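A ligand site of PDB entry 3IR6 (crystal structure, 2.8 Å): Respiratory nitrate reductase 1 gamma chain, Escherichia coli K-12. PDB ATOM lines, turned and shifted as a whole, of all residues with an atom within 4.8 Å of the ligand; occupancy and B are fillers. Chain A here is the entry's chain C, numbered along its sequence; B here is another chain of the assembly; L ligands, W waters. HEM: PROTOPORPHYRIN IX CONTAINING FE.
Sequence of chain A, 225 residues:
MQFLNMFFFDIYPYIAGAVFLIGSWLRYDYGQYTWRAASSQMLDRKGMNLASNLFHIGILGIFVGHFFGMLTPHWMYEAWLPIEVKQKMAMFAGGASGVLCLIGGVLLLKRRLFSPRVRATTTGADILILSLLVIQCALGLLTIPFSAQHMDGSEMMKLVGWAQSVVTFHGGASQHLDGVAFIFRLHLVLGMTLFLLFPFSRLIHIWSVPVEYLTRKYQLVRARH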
ATOM      1  N   ALA A  37      -0.534  11.378 -21.058  1.00  0.00           N
ATOM      2  CA  ALA A  37      -1.636  11.980 -21.795  1.00  0.00           C
ATOM      3  C   ALA A  37      -1.197  12.422 -23.180  1.00  0.00           C
ATOM      4  O   ALA A  37      -2.024  12.682 -24.056  1.00  0.00           O
ATOM      5  CB  ALA A  37      -2.195  13.148 -21.037  1.00  0.00           C
ATOM      6  N   ALA A  38       0.113  12.514 -23.383  1.00  0.00           N
ATOM      7  CA  ALA A  38       0.656  12.912 -24.678  1.00  0.00           C
ATOM      8  C   ALA A  38       0.175  14.266 -25.150  1.00  0.00           C
ATOM      9  O   ALA A  38      -0.396  14.379 -26.240  1.00  0.00           O
ATOM     10  CB  ALA A  38       0.293  11.862 -25.716  1.00  0.00           C
ATOM     11  N   SER A  39       0.396  15.302 -24.356  1.00  0.00           N
ATOM     12  CA  SER A  39      -0.020  16.631 -24.742  1.00  0.00           C
ATOM     13  C   SER A  39       0.652  17.109 -26.024  1.00  0.00           C
ATOM     14  O   SER A  39       1.823  16.859 -26.267  1.00  0.00           O
ATOM     15  CB  SER A  39       0.291  17.623 -23.617  1.00  0.00           C
ATOM     16  OG  SER A  39       0.239  18.949 -24.111  1.00  0.00           O
ATOM     17  N   SER A  40      -0.096  17.823 -26.856  1.00  0.00           N
ATOM     18  CA  SER A  40       0.448  18.348 -28.091  1.00  0.00           C
ATOM     19  C   SER A  40       0.315  19.861 -28.026  1.00  0.00           C
ATOM     20  O   SER A  40       0.773  20.559 -28.915  1.00  0.00           O
ATOM     21  CB  SER A  40      -0.316  17.813 -29.313  1.00  0.00           C
ATOM     22  OG  SER A  40      -1.686  18.175 -29.285  1.00  0.00           O
ATOM     23  N   GLN A  41      -0.286  20.346 -26.953  1.00  0.00           N
ATOM     24  CA  GLN A  41      -0.536  21.769 -26.779  1.00  0.00           C
ATOM     25  C   GLN A  41       0.647  22.698 -27.102  1.00  0.00           C
ATOM     26  O   GLN A  41       0.496  23.677 -27.827  1.00  0.00           O
ATOM     27  CB  GLN A  41      -0.992  22.046 -25.352  1.00  0.00           C
ATOM     28  CG  GLN A  41      -1.666  23.403 -25.173  1.00  0.00           C
ATOM     29  CD  GLN A  41      -1.859  23.770 -23.711  1.00  0.00           C
ATOM     30  OE1 GLN A  41      -1.881  22.898 -22.827  1.00  0.00           O
ATOM     31  NE2 GLN A  41      -2.016  25.056 -23.444  1.00  0.00           N
ATOM     32  N   MET A  48      -6.728  25.352 -28.800  1.00  0.00           N
ATOM     33  CA  MET A  48      -6.643  24.252 -27.840  1.00  0.00           C
ATOM     34  C   MET A  48      -7.414  24.501 -26.576  1.00  0.00           C
ATOM     35  O   MET A  48      -8.006  23.580 -26.004  1.00  0.00           O
ATOM     36  CB  MET A  48      -5.190  23.942 -27.498  1.00  0.00           C
ATOM     37  CG  MET A  48      -4.584  22.964 -28.449  1.00  0.00           C
ATOM     38  SD  MET A  48      -5.543  21.439 -28.445  1.00  0.00           S
ATOM     39  CE  MET A  48      -4.581  20.487 -27.290  1.00  0.00           C
ATOM     40  N   SER A  52     -10.185  21.703 -26.504  1.00  0.00           N
ATOM     41  CA  SER A  52      -9.960  20.650 -25.520  1.00  0.00           C
ATOM     42  C   SER A  52     -10.931  20.737 -24.346  1.00  0.00           C
ATOM     43  O   SER A  52     -11.417  19.699 -23.874  1.00  0.00           O
ATOM     44  CB  SER A  52      -8.510  20.686 -25.000  1.00  0.00           C
ATOM     45  OG  SER A  52      -8.283  19.663 -24.038  1.00  0.00           O
ATOM     46  N   PHE A  55     -14.401  19.528 -25.530  1.00  0.00           N
ATOM     47  CA  PHE A  55     -14.347  18.087 -25.604  1.00  0.00           C
ATOM     48  C   PHE A  55     -14.350  17.386 -24.239  1.00  0.00           C
ATOM     49  O   PHE A  55     -15.216  16.544 -23.975  1.00  0.00           O
ATOM     50  CB  PHE A  55     -13.134  17.644 -26.439  1.00  0.00           C
ATOM     51  CG  PHE A  55     -12.901  16.153 -26.415  1.00  0.00           C
ATOM     52  CD1 PHE A  55     -12.079  15.586 -25.455  1.00  0.00           C
ATOM     53  CD2 PHE A  55     -13.559  15.324 -27.309  1.00  0.00           C
ATOM     54  CE1 PHE A  55     -11.922  14.204 -25.376  1.00  0.00           C
ATOM     55  CE2 PHE A  55     -13.409  13.936 -27.253  1.00  0.00           C
ATOM     56  CZ  PHE A  55     -12.591  13.375 -26.281  1.00  0.00           C
ATOM     57  N   HIS A  56     -13.405  17.721 -23.371  1.00  0.00           N
ATOM     58  CA  HIS A  56     -13.346  17.073 -22.064  1.00  0.00           C
ATOM     59  C   HIS A  56     -14.518  17.313 -21.134  1.00  0.00           C
ATOM     60  O   HIS A  56     -14.950  16.415 -20.431  1.00  0.00           O
ATOM     61  CB  HIS A  56     -12.044  17.429 -21.319  1.00  0.00           C
ATOM     62  CG  HIS A  56     -10.854  16.645 -21.767  1.00  0.00           C
ATOM     63  ND1 HIS A  56      -9.946  17.135 -22.681  1.00  0.00           N
ATOM     64  CD2 HIS A  56     -10.493  15.357 -21.514  1.00  0.00           C
ATOM     65  CE1 HIS A  56      -9.073  16.183 -22.979  1.00  0.00           C
ATOM     66  NE2 HIS A  56      -9.384  15.099 -22.282  1.00  0.00           N
ATOM     67  N   ILE A  59     -17.357  15.268 -22.756  1.00  0.00           N
ATOM     68  CA  ILE A  59     -17.127  13.854 -22.551  1.00  0.00           C
ATOM     69  C   ILE A  59     -17.340  13.445 -21.095  1.00  0.00           C
ATOM     70  O   ILE A  59     -17.821  12.354 -20.806  1.00  0.00           O
ATOM     71  CB  ILE A  59     -15.691  13.459 -23.008  1.00  0.00           C
ATOM     72  CG1 ILE A  59     -15.625  11.953 -23.289  1.00  0.00           C
ATOM     73  CG2 ILE A  59     -14.674  13.808 -21.949  1.00  0.00           C
ATOM     74  CD1 ILE A  59     -16.140  11.565 -24.637  1.00  0.00           C
ATOM     75  N   LEU A  60     -16.993  14.333 -20.169  1.00  0.00           N
ATOM     76  CA  LEU A  60     -17.159  14.013 -18.759  1.00  0.00           C
ATOM     77  C   LEU A  60     -18.634  14.023 -18.336  1.00  0.00           C
ATOM     78  O   LEU A  60     -19.039  13.243 -17.472  1.00  0.00           O
ATOM     79  CB  LEU A  60     -16.318  14.969 -17.901  1.00  0.00           C
ATOM     80  CG  LEU A  60     -14.835  14.557 -17.914  1.00  0.00           C
ATOM     81  CD1 LEU A  60     -13.961  15.667 -17.406  1.00  0.00           C
ATOM     82  CD2 LEU A  60     -14.664  13.332 -17.055  1.00  0.00           C
ATOM     83  N   LEU A 108     -10.628  19.405 -32.396  1.00  0.00           N
ATOM     84  CA  LEU A 108      -9.359  18.756 -32.093  1.00  0.00           C
ATOM     85  C   LEU A 108      -8.919  17.851 -33.240  1.00  0.00           C
ATOM     86  O   LEU A 108      -7.726  17.763 -33.549  1.00  0.00           O
ATOM     87  CB  LEU A 108      -9.464  17.921 -30.820  1.00  0.00           C
ATOM     88  CG  LEU A 108      -9.498  18.724 -29.519  1.00  0.00           C
ATOM     89  CD1 LEU A 108      -9.873  17.811 -28.372  1.00  0.00           C
ATOM     90  CD2 LEU A 108      -8.142  19.371 -29.292  1.00  0.00           C
ATOM     91  N   ARG A 111      -7.620  19.822 -36.111  1.00  0.00           N
ATOM     92  CA  ARG A 111      -6.274  20.209 -35.702  1.00  0.00           C
ATOM     93  C   ARG A 111      -5.241  19.103 -35.881  1.00  0.00           C
ATOM     94  O   ARG A 111      -4.234  19.312 -36.558  1.00  0.00           O
ATOM     95  CB  ARG A 111      -6.296  20.661 -34.226  1.00  0.00           C
ATOM     96  CG  ARG A 111      -4.935  21.080 -33.651  1.00  0.00           C
ATOM     97  CD  ARG A 111      -5.134  21.700 -32.289  1.00  0.00           C
ATOM     98  NE  ARG A 111      -3.904  21.863 -31.519  1.00  0.00           N
ATOM     99  CZ  ARG A 111      -3.176  20.859 -31.036  1.00  0.00           C
ATOM    100  NH1 ARG A 111      -2.070  21.120 -30.340  1.00  0.00           N
ATOM    101  NH2 ARG A 111      -3.536  19.598 -31.240  1.00  0.00           N
ATOM    102  N   ARG A 112      -5.498  17.929 -35.295  1.00  0.00           N
ATOM    103  CA  ARG A 112      -4.572  16.805 -35.405  1.00  0.00           C
ATOM    104  C   ARG A 112      -4.240  16.458 -36.831  1.00  0.00           C
ATOM    105  O   ARG A 112      -3.110  16.102 -37.148  1.00  0.00           O
ATOM    106  CB  ARG A 112      -5.150  15.573 -34.709  1.00  0.00           C
ATOM    107  CG  ARG A 112      -4.286  14.320 -34.806  1.00  0.00           C
ATOM    108  CD  ARG A 112      -4.667  13.320 -33.706  1.00  0.00           C
ATOM    109  NE  ARG A 112      -4.432  13.936 -32.402  1.00  0.00           N
ATOM    110  CZ  ARG A 112      -3.216  14.153 -31.897  1.00  0.00           C
ATOM    111  NH1 ARG A 112      -2.142  13.792 -32.592  1.00  0.00           N
ATOM    112  NH2 ARG A 112      -3.063  14.771 -30.738  1.00  0.00           N
ATOM    113  N   ILE A 129      -8.181   6.671 -32.470  1.00  0.00           N
ATOM    114  CA  ILE A 129      -8.912   6.878 -31.240  1.00  0.00           C
ATOM    115  C   ILE A 129      -9.779   8.130 -31.217  1.00  0.00           C
ATOM    116  O   ILE A 129     -10.925   8.103 -30.766  1.00  0.00           O
ATOM    117  CB  ILE A 129      -7.938   6.831 -30.040  1.00  0.00           C
ATOM    118  CG1 ILE A 129      -8.120   5.499 -29.315  1.00  0.00           C
ATOM    119  CG2 ILE A 129      -8.152   7.996 -29.088  1.00  0.00           C
ATOM    120  CD1 ILE A 129      -9.552   5.236 -28.891  1.00  0.00           C
ATOM    121  N   LEU A 130      -9.247   9.227 -31.714  1.00  0.00           N
ATOM    122  CA  LEU A 130     -10.003  10.473 -31.714  1.00  0.00           C
ATOM    123  C   LEU A 130     -11.126  10.405 -32.729  1.00  0.00           C
ATOM    124  O   LEU A 130     -12.158  11.037 -32.569  1.00  0.00           O
ATOM    125  CB  LEU A 130      -9.095  11.639 -32.068  1.00  0.00           C
ATOM    126  CG  LEU A 130      -9.856  12.955 -32.047  1.00  0.00           C
ATOM    127  CD1 LEU A 130     -10.252  13.237 -30.598  1.00  0.00           C
ATOM    128  CD2 LEU A 130      -9.025  14.079 -32.653  1.00  0.00           C
ATOM    129  N   LEU A 133     -14.164   8.201 -31.261  1.00  0.00           N
ATOM    130  CA  LEU A 133     -14.936   8.944 -30.265  1.00  0.00           C
ATOM    131  C   LEU A 133     -15.823   9.998 -30.929  1.00  0.00           C
ATOM    132  O   LEU A 133     -16.964  10.207 -30.511  1.00  0.00           O
ATOM    133  CB  LEU A 133     -14.003   9.634 -29.258  1.00  0.00           C
ATOM    134  CG  LEU A 133     -13.223   8.806 -28.231  1.00  0.00           C
ATOM    135  CD1 LEU A 133     -12.047   9.622 -27.763  1.00  0.00           C
ATOM    136  CD2 LEU A 133     -14.100   8.392 -27.053  1.00  0.00           C
ATOM    137  N   ARG A 202      -3.982   6.223 -26.037  1.00  0.00           N
ATOM    138  CA  ARG A 202      -3.694   7.266 -25.074  1.00  0.00           C
ATOM    139  C   ARG A 202      -4.745   7.298 -23.968  1.00  0.00           C
ATOM    140  O   ARG A 202      -4.507   7.848 -22.882  1.00  0.00           O
ATOM    141  CB  ARG A 202      -3.655   8.608 -25.794  1.00  0.00           C
ATOM    142  CG  ARG A 202      -5.005   9.047 -26.349  1.00  0.00           C
ATOM    143  CD  ARG A 202      -4.864  10.225 -27.277  1.00  0.00           C
ATOM    144  NE  ARG A 202      -4.186  11.333 -26.611  1.00  0.00           N
ATOM    145  CZ  ARG A 202      -3.652  12.368 -27.231  1.00  0.00           C
ATOM    146  NH1 ARG A 202      -3.697  12.446 -28.556  1.00  0.00           N
ATOM    147  NH2 ARG A 202      -3.077  13.337 -26.533  1.00  0.00           N
ATOM    148  N   LEU A 203      -5.917   6.710 -24.230  1.00  0.00           N
ATOM    149  CA  LEU A 203      -7.004   6.700 -23.251  1.00  0.00           C
ATOM    150  C   LEU A 203      -6.611   6.252 -21.844  1.00  0.00           C
ATOM    151  O   LEU A 203      -7.353   6.511 -20.902  1.00  0.00           O
ATOM    152  CB  LEU A 203      -8.185   5.851 -23.761  1.00  0.00           C
ATOM    153  CG  LEU A 203      -8.836   6.366 -25.062  1.00  0.00           C
ATOM    154  CD1 LEU A 203     -10.162   5.665 -25.295  1.00  0.00           C
ATOM    155  CD2 LEU A 203      -9.082   7.861 -24.970  1.00  0.00           C
ATOM    156  N   HIS A 205      -4.809   7.624 -19.926  1.00  0.00           N
ATOM    157  CA  HIS A 205      -4.620   8.787 -19.041  1.00  0.00           C
ATOM    158  C   HIS A 205      -5.794   8.909 -18.094  1.00  0.00           C
ATOM    159  O   HIS A 205      -5.659   9.409 -16.971  1.00  0.00           O
ATOM    160  CB  HIS A 205      -4.406  10.108 -19.832  1.00  0.00           C
ATOM    161  CG  HIS A 205      -5.600  10.613 -20.588  1.00  0.00           C
ATOM    162  ND1 HIS A 205      -6.193   9.905 -21.613  1.00  0.00           N
ATOM    163  CD2 HIS A 205      -6.215  11.819 -20.570  1.00  0.00           C
ATOM    164  CE1 HIS A 205      -7.107  10.657 -22.202  1.00  0.00           C
ATOM    165  NE2 HIS A 205      -7.141  11.830 -21.594  1.00  0.00           N
ATOM    166  N   ILE A 206      -6.930   8.397 -18.554  1.00  0.00           N
ATOM    167  CA  ILE A 206      -8.151   8.431 -17.780  1.00  0.00           C
ATOM    168  C   ILE A 206      -8.016   7.762 -16.417  1.00  0.00           C
ATOM    169  O   ILE A 206      -8.561   8.266 -15.443  1.00  0.00           O
ATOM    170  CB  ILE A 206      -9.282   7.794 -18.591  1.00  0.00           C
ATOM    171  CG1 ILE A 206      -9.380   8.507 -19.941  1.00  0.00           C
ATOM    172  CG2 ILE A 206     -10.607   7.913 -17.822  1.00  0.00           C
ATOM    173  CD1 ILE A 206     -10.464   7.967 -20.828  1.00  0.00           C
ATOM    174  N   VAL A 209      -6.575  10.170 -13.532  1.00  0.00           N
ATOM    175  CA  VAL A 209      -7.224  11.401 -13.057  1.00  0.00           C
ATOM    176  C   VAL A 209      -6.617  11.702 -11.674  1.00  0.00           C
ATOM    177  O   VAL A 209      -6.765  10.926 -10.718  1.00  0.00           O
ATOM    178  CB  VAL A 209      -8.761  11.206 -12.988  1.00  0.00           C
ATOM    179  CG1 VAL A 209      -9.091   9.851 -12.415  1.00  0.00           C
ATOM    180  CG2 VAL A 209      -9.396  12.293 -12.139  1.00  0.00           C
ATOM    181  N   PRO A 210      -5.930  12.844 -11.542  1.00  0.00           N
ATOM    182  CA  PRO A 210      -5.249  13.316 -10.327  1.00  0.00           C
ATOM    183  C   PRO A 210      -6.109  13.744  -9.144  1.00  0.00           C
ATOM    184  O   PRO A 210      -5.888  14.814  -8.569  1.00  0.00           O
ATOM    185  CB  PRO A 210      -4.406  14.471 -10.840  1.00  0.00           C
ATOM    186  CG  PRO A 210      -5.357  15.104 -11.810  1.00  0.00           C
ATOM    187  CD  PRO A 210      -5.943  13.913 -12.565  1.00  0.00           C
ATOM    188  N   ILE B  88      -6.405  21.896 -16.266  1.00  0.00           N
ATOM    189  CA  ILE B  88      -5.768  20.718 -16.818  1.00  0.00           C
ATOM    190  C   ILE B  88      -6.048  20.328 -18.262  1.00  0.00           C
ATOM    191  O   ILE B  88      -5.142  19.867 -18.954  1.00  0.00           O
ATOM    192  CB  ILE B  88      -6.024  19.506 -15.889  1.00  0.00           C
ATOM    193  CG1 ILE B  88      -4.969  18.418 -16.135  1.00  0.00           C
ATOM    194  CG2 ILE B  88      -7.425  18.950 -16.108  1.00  0.00           C
ATOM    195  CD1 ILE B  88      -4.713  17.543 -14.930  1.00  0.00           C
ATOM    196  N   PHE B  89      -7.275  20.490 -18.745  1.00  0.00           N
ATOM    197  CA  PHE B  89      -7.549  20.092 -20.119  1.00  0.00           C
ATOM    198  C   PHE B  89      -6.813  20.992 -21.095  1.00  0.00           C
ATOM    199  O   PHE B  89      -6.695  20.667 -22.283  1.00  0.00           O
ATOM    200  CB  PHE B  89      -9.052  20.111 -20.413  1.00  0.00           C
ATOM    201  CG  PHE B  89      -9.850  19.349 -19.415  1.00  0.00           C
ATOM    202  CD1 PHE B  89      -9.498  18.058 -19.059  1.00  0.00           C
ATOM    203  CD2 PHE B  89     -10.950  19.926 -18.801  1.00  0.00           C
ATOM    204  CE1 PHE B  89     -10.238  17.351 -18.097  1.00  0.00           C
ATOM    205  CE2 PHE B  89     -11.693  19.228 -17.836  1.00  0.00           C
ATOM    206  CZ  PHE B  89     -11.332  17.944 -17.488  1.00  0.00           C
ATOM    207  N   TRP B 220       0.882  15.775 -17.379  1.00  0.00           N
ATOM    208  CA  TRP B 220      -0.190  16.724 -17.101  1.00  0.00           C
ATOM    209  C   TRP B 220       0.277  18.128 -17.410  1.00  0.00           C
ATOM    210  O   TRP B 220      -0.513  19.069 -17.367  1.00  0.00           O
ATOM    211  CB  TRP B 220      -0.621  16.685 -15.636  1.00  0.00           C
ATOM    212  CG  TRP B 220      -1.241  15.400 -15.185  1.00  0.00           C
ATOM    213  CD1 TRP B 220      -0.960  14.710 -14.039  1.00  0.00           C
ATOM    214  CD2 TRP B 220      -2.245  14.640 -15.868  1.00  0.00           C
ATOM    215  NE1 TRP B 220      -1.724  13.574 -13.960  1.00  0.00           N
ATOM    216  CE2 TRP B 220      -2.526  13.504 -15.072  1.00  0.00           C
ATOM    217  CE3 TRP B 220      -2.936  14.820 -17.072  1.00  0.00           C
ATOM    218  CZ2 TRP B 220      -3.466  12.540 -15.451  1.00  0.00           C
ATOM    219  CZ3 TRP B 220      -3.875  13.854 -17.441  1.00  0.00           C
ATOM    220  CH2 TRP B 220      -4.128  12.725 -16.633  1.00  0.00           C
ATOM    221  N   ARG B 221       1.564  18.252 -17.707  1.00  0.00           N
ATOM    222  CA  ARG B 221       2.210  19.523 -18.047  1.00  0.00           C
ATOM    223  C   ARG B 221       1.768  20.783 -17.294  1.00  0.00           C
ATOM    224  O   ARG B 221       1.580  21.835 -17.902  1.00  0.00           O
ATOM    225  CB  ARG B 221       2.094  19.760 -19.542  1.00  0.00           C
ATOM    226  CG  ARG B 221       0.680  19.599 -20.081  1.00  0.00           C
ATOM    227  CD  ARG B 221       0.123  20.879 -20.700  1.00  0.00           C
ATOM    228  NE  ARG B 221      -1.200  20.651 -21.270  1.00  0.00           N
ATOM    229  CZ  ARG B 221      -2.266  20.326 -20.544  1.00  0.00           C
ATOM    230  NH1 ARG B 221      -2.159  20.195 -19.226  1.00  0.00           N
ATOM    231  NH2 ARG B 221      -3.431  20.112 -21.142  1.00  0.00           N
HETATM  232  CHA HEM L   1      -6.153  14.474 -24.289  1.00  0.00           C
HETATM  233  CHB HEM L   1      -6.492  15.227 -19.551  1.00  0.00           C
HETATM  234  CHC HEM L   1     -10.453  12.432 -19.541  1.00  0.00           C
HETATM  235  CHD HEM L   1     -10.075  11.656 -24.265  1.00  0.00           C
HETATM  236  C1A HEM L   1      -5.886  14.925 -23.025  1.00  0.00           C
HETATM  237  C2A HEM L   1      -4.788  15.795 -22.613  1.00  0.00           C
HETATM  238  C3A HEM L   1      -4.871  16.017 -21.300  1.00  0.00           C
HETATM  239  C4A HEM L   1      -6.049  15.274 -20.847  1.00  0.00           C
HETATM  240  CMA HEM L   1      -3.954  16.855 -20.363  1.00  0.00           C
HETATM  241  CAA HEM L   1      -3.727  16.350 -23.582  1.00  0.00           C
HETATM  242  CBA HEM L   1      -4.184  17.755 -24.153  1.00  0.00           C
HETATM  243  CGA HEM L   1      -3.076  18.574 -24.834  1.00  0.00           C
HETATM  244  O1A HEM L   1      -2.543  19.484 -24.143  1.00  0.00           O
HETATM  245  O2A HEM L   1      -2.770  18.238 -26.037  1.00  0.00           O
HETATM  246  C1B HEM L   1      -7.607  14.525 -19.117  1.00  0.00           C
HETATM  247  C2B HEM L   1      -8.089  14.468 -17.729  1.00  0.00           C
HETATM  248  C3B HEM L   1      -9.216  13.683 -17.728  1.00  0.00           C
HETATM  249  C4B HEM L   1      -9.423  13.248 -19.113  1.00  0.00           C
HETATM  250  CMB HEM L   1      -7.355  15.221 -16.565  1.00  0.00           C
HETATM  251  CAB HEM L   1     -10.171  13.243 -16.526  1.00  0.00           C
HETATM  252  CBB HEM L   1     -10.034  13.593 -15.208  1.00  0.00           C
HETATM  253  C1C HEM L   1     -10.716  11.975 -20.817  1.00  0.00           C
HETATM  254  C2C HEM L   1     -11.840  11.113 -21.216  1.00  0.00           C
HETATM  255  C3C HEM L   1     -11.716  10.898 -22.537  1.00  0.00           C
HETATM  256  C4C HEM L   1     -10.532  11.617 -22.977  1.00  0.00           C
HETATM  257  CMC HEM L   1     -12.940  10.572 -20.232  1.00  0.00           C
HETATM  258  CAC HEM L   1     -12.612  10.069 -23.514  1.00  0.00           C
HETATM  259  CBC HEM L   1     -12.337   8.744 -23.648  1.00  0.00           C
HETATM  260  C1D HEM L   1      -8.969  12.352 -24.691  1.00  0.00           C
HETATM  261  C2D HEM L   1      -8.487  12.375 -26.078  1.00  0.00           C
HETATM  262  C3D HEM L   1      -7.411  13.183 -26.072  1.00  0.00           C
HETATM  263  C4D HEM L   1      -7.189  13.636 -24.691  1.00  0.00           C
HETATM  264  CMD HEM L   1      -9.144  11.627 -27.272  1.00  0.00           C
HETATM  265  CAD HEM L   1      -6.450  13.645 -27.194  1.00  0.00           C
HETATM  266  CBD HEM L   1      -6.925  14.942 -27.944  1.00  0.00           C
HETATM  267  CGD HEM L   1      -6.030  15.278 -29.136  1.00  0.00           C
HETATM  268  O1D HEM L   1      -4.939  15.911 -28.869  1.00  0.00           O
HETATM  269  O2D HEM L   1      -6.479  14.885 -30.276  1.00  0.00           O
HETATM  270  NA  HEM L   1      -6.653  14.614 -21.931  1.00  0.00           N
HETATM  271  NB  HEM L   1      -8.437  13.763 -19.937  1.00  0.00           N
HETATM  272  NC  HEM L   1      -9.937  12.280 -21.913  1.00  0.00           N
HETATM  273  ND  HEM L   1      -8.144  13.125 -23.877  1.00  0.00           N
HETATM  274 FE   HEM L   1      -8.267  13.461 -21.933  1.00  0.00          FE
HETATM  275  O   HOH W   1      -6.226  12.019 -30.221  1.00  0.00           O
HETATM  276  O   HOH W   2      -4.687  11.654 -23.937  1.00  0.00           O
HETATM  277  O   HOH W   3      -5.627  17.880 -31.493  1.00  0.00           O
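Merely in contact with the ligand: Ala 37, Met 48, Phe 55, Ile 59, Leu 130, Leu 133, Leu 203, Ile 206, Val 209, Ile 88 of chain B, Phe 89 of chain B and Trp 220 of chain B. Hydrophobic or aromatic side chains within 4 Å of the ligand: Ala 37, Met 48, Phe 55, His 56, Ile 59, Leu 130, Leu 133, Leu 203, His 205, Ile 206, Val 209, Ile 88 of chain B, Phe 89 of chain B and Trp 220 of chain B.
Water W1 lies within hydrogen-bond range of O2D of the ligand (2.9 Å), NH1 of Arg 202 (3.1 Å) and NE of Arg 112 (3.4 Å). Water W2 lies within hydrogen-bond range of the guanidinium group (NE) of Arg 202, the backbone carbonyl oxygen (O) of Ala 37 and a ring nitrogen (ND1) of His 205. Water W3 lies within hydrogen-bond range of NH2 of Arg 111 (2.7 Å), O of Leu 108 (2.9 Å) and O2D of the ligand (3.3 Å).
A ring nitrogen (ND1) of His 205 is in hydrogen-bond range of the backbone carbonyl oxygen of Arg 202 (2.9 Å). The side-chain hydroxyl (OG) of Ser 39 is in hydrogen-bond range of the backbone NH (N) of Gln 41, 3.2 Å away. NH2 of Arg 221 of chain B is in hydrogen-bond range of O of Ile 88 of chain B (2.8 Å). NH2 of Arg 111 lies within hydrogen-bond range of OG of Ser 40 (3.0 Å). The guanidinium group (NE) of Arg 221 of chain B sits at hydrogen-bond distance from the side-chain amide oxygen (OE1) of Gln 41 (2.8 Å). OG of Ser 52 lies within hydrogen-bond range of O of Phe 89 of chain B (2.6 Å). The guanidinium group of Arg 202 lies within hydrogen-bond range of the backbone carbonyl oxygen of Ala 37 (2.8 Å). ND1 of His 56 lies within hydrogen-bond range of O of Ser 52 (3.2 Å).
An oxygen (O1A) of the ligand lies within salt-bridge range of the guanidinium group (NH2) of Arg 221 of chain B (3.2 Å). An oxygen (O2A) of the ligand lies within hydrogen-bond range of the side-chain hydroxyl (OG) of Ser 40 (3.4 Å). The backbone NH (N) of Gln 41 sits at hydrogen-bond distance from an oxygen (O2A) of the ligand, at 3.4 Å. The side-chain hydroxyl (OG) of Ser 39 sits at hydrogen-bond distance from an oxygen (O1A) of the ligand. NE2 of His 56 is bound to FE of the ligand (2.0 Å). The backbone NH (N) of Ser 40 sits at hydrogen-bond distance from an oxygen (O2A) of the ligand (2.8 Å). O1D of the ligand is in salt-bridge range of NH2 of Arg 112, 2.9 Å away. An iron atom (FE) of the ligand is bound by a ring nitrogen (NE2) of His 205 (2.0 Å). O1D of the ligand lies within salt-bridge range of NH1 of Arg 202 (3.7 Å).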
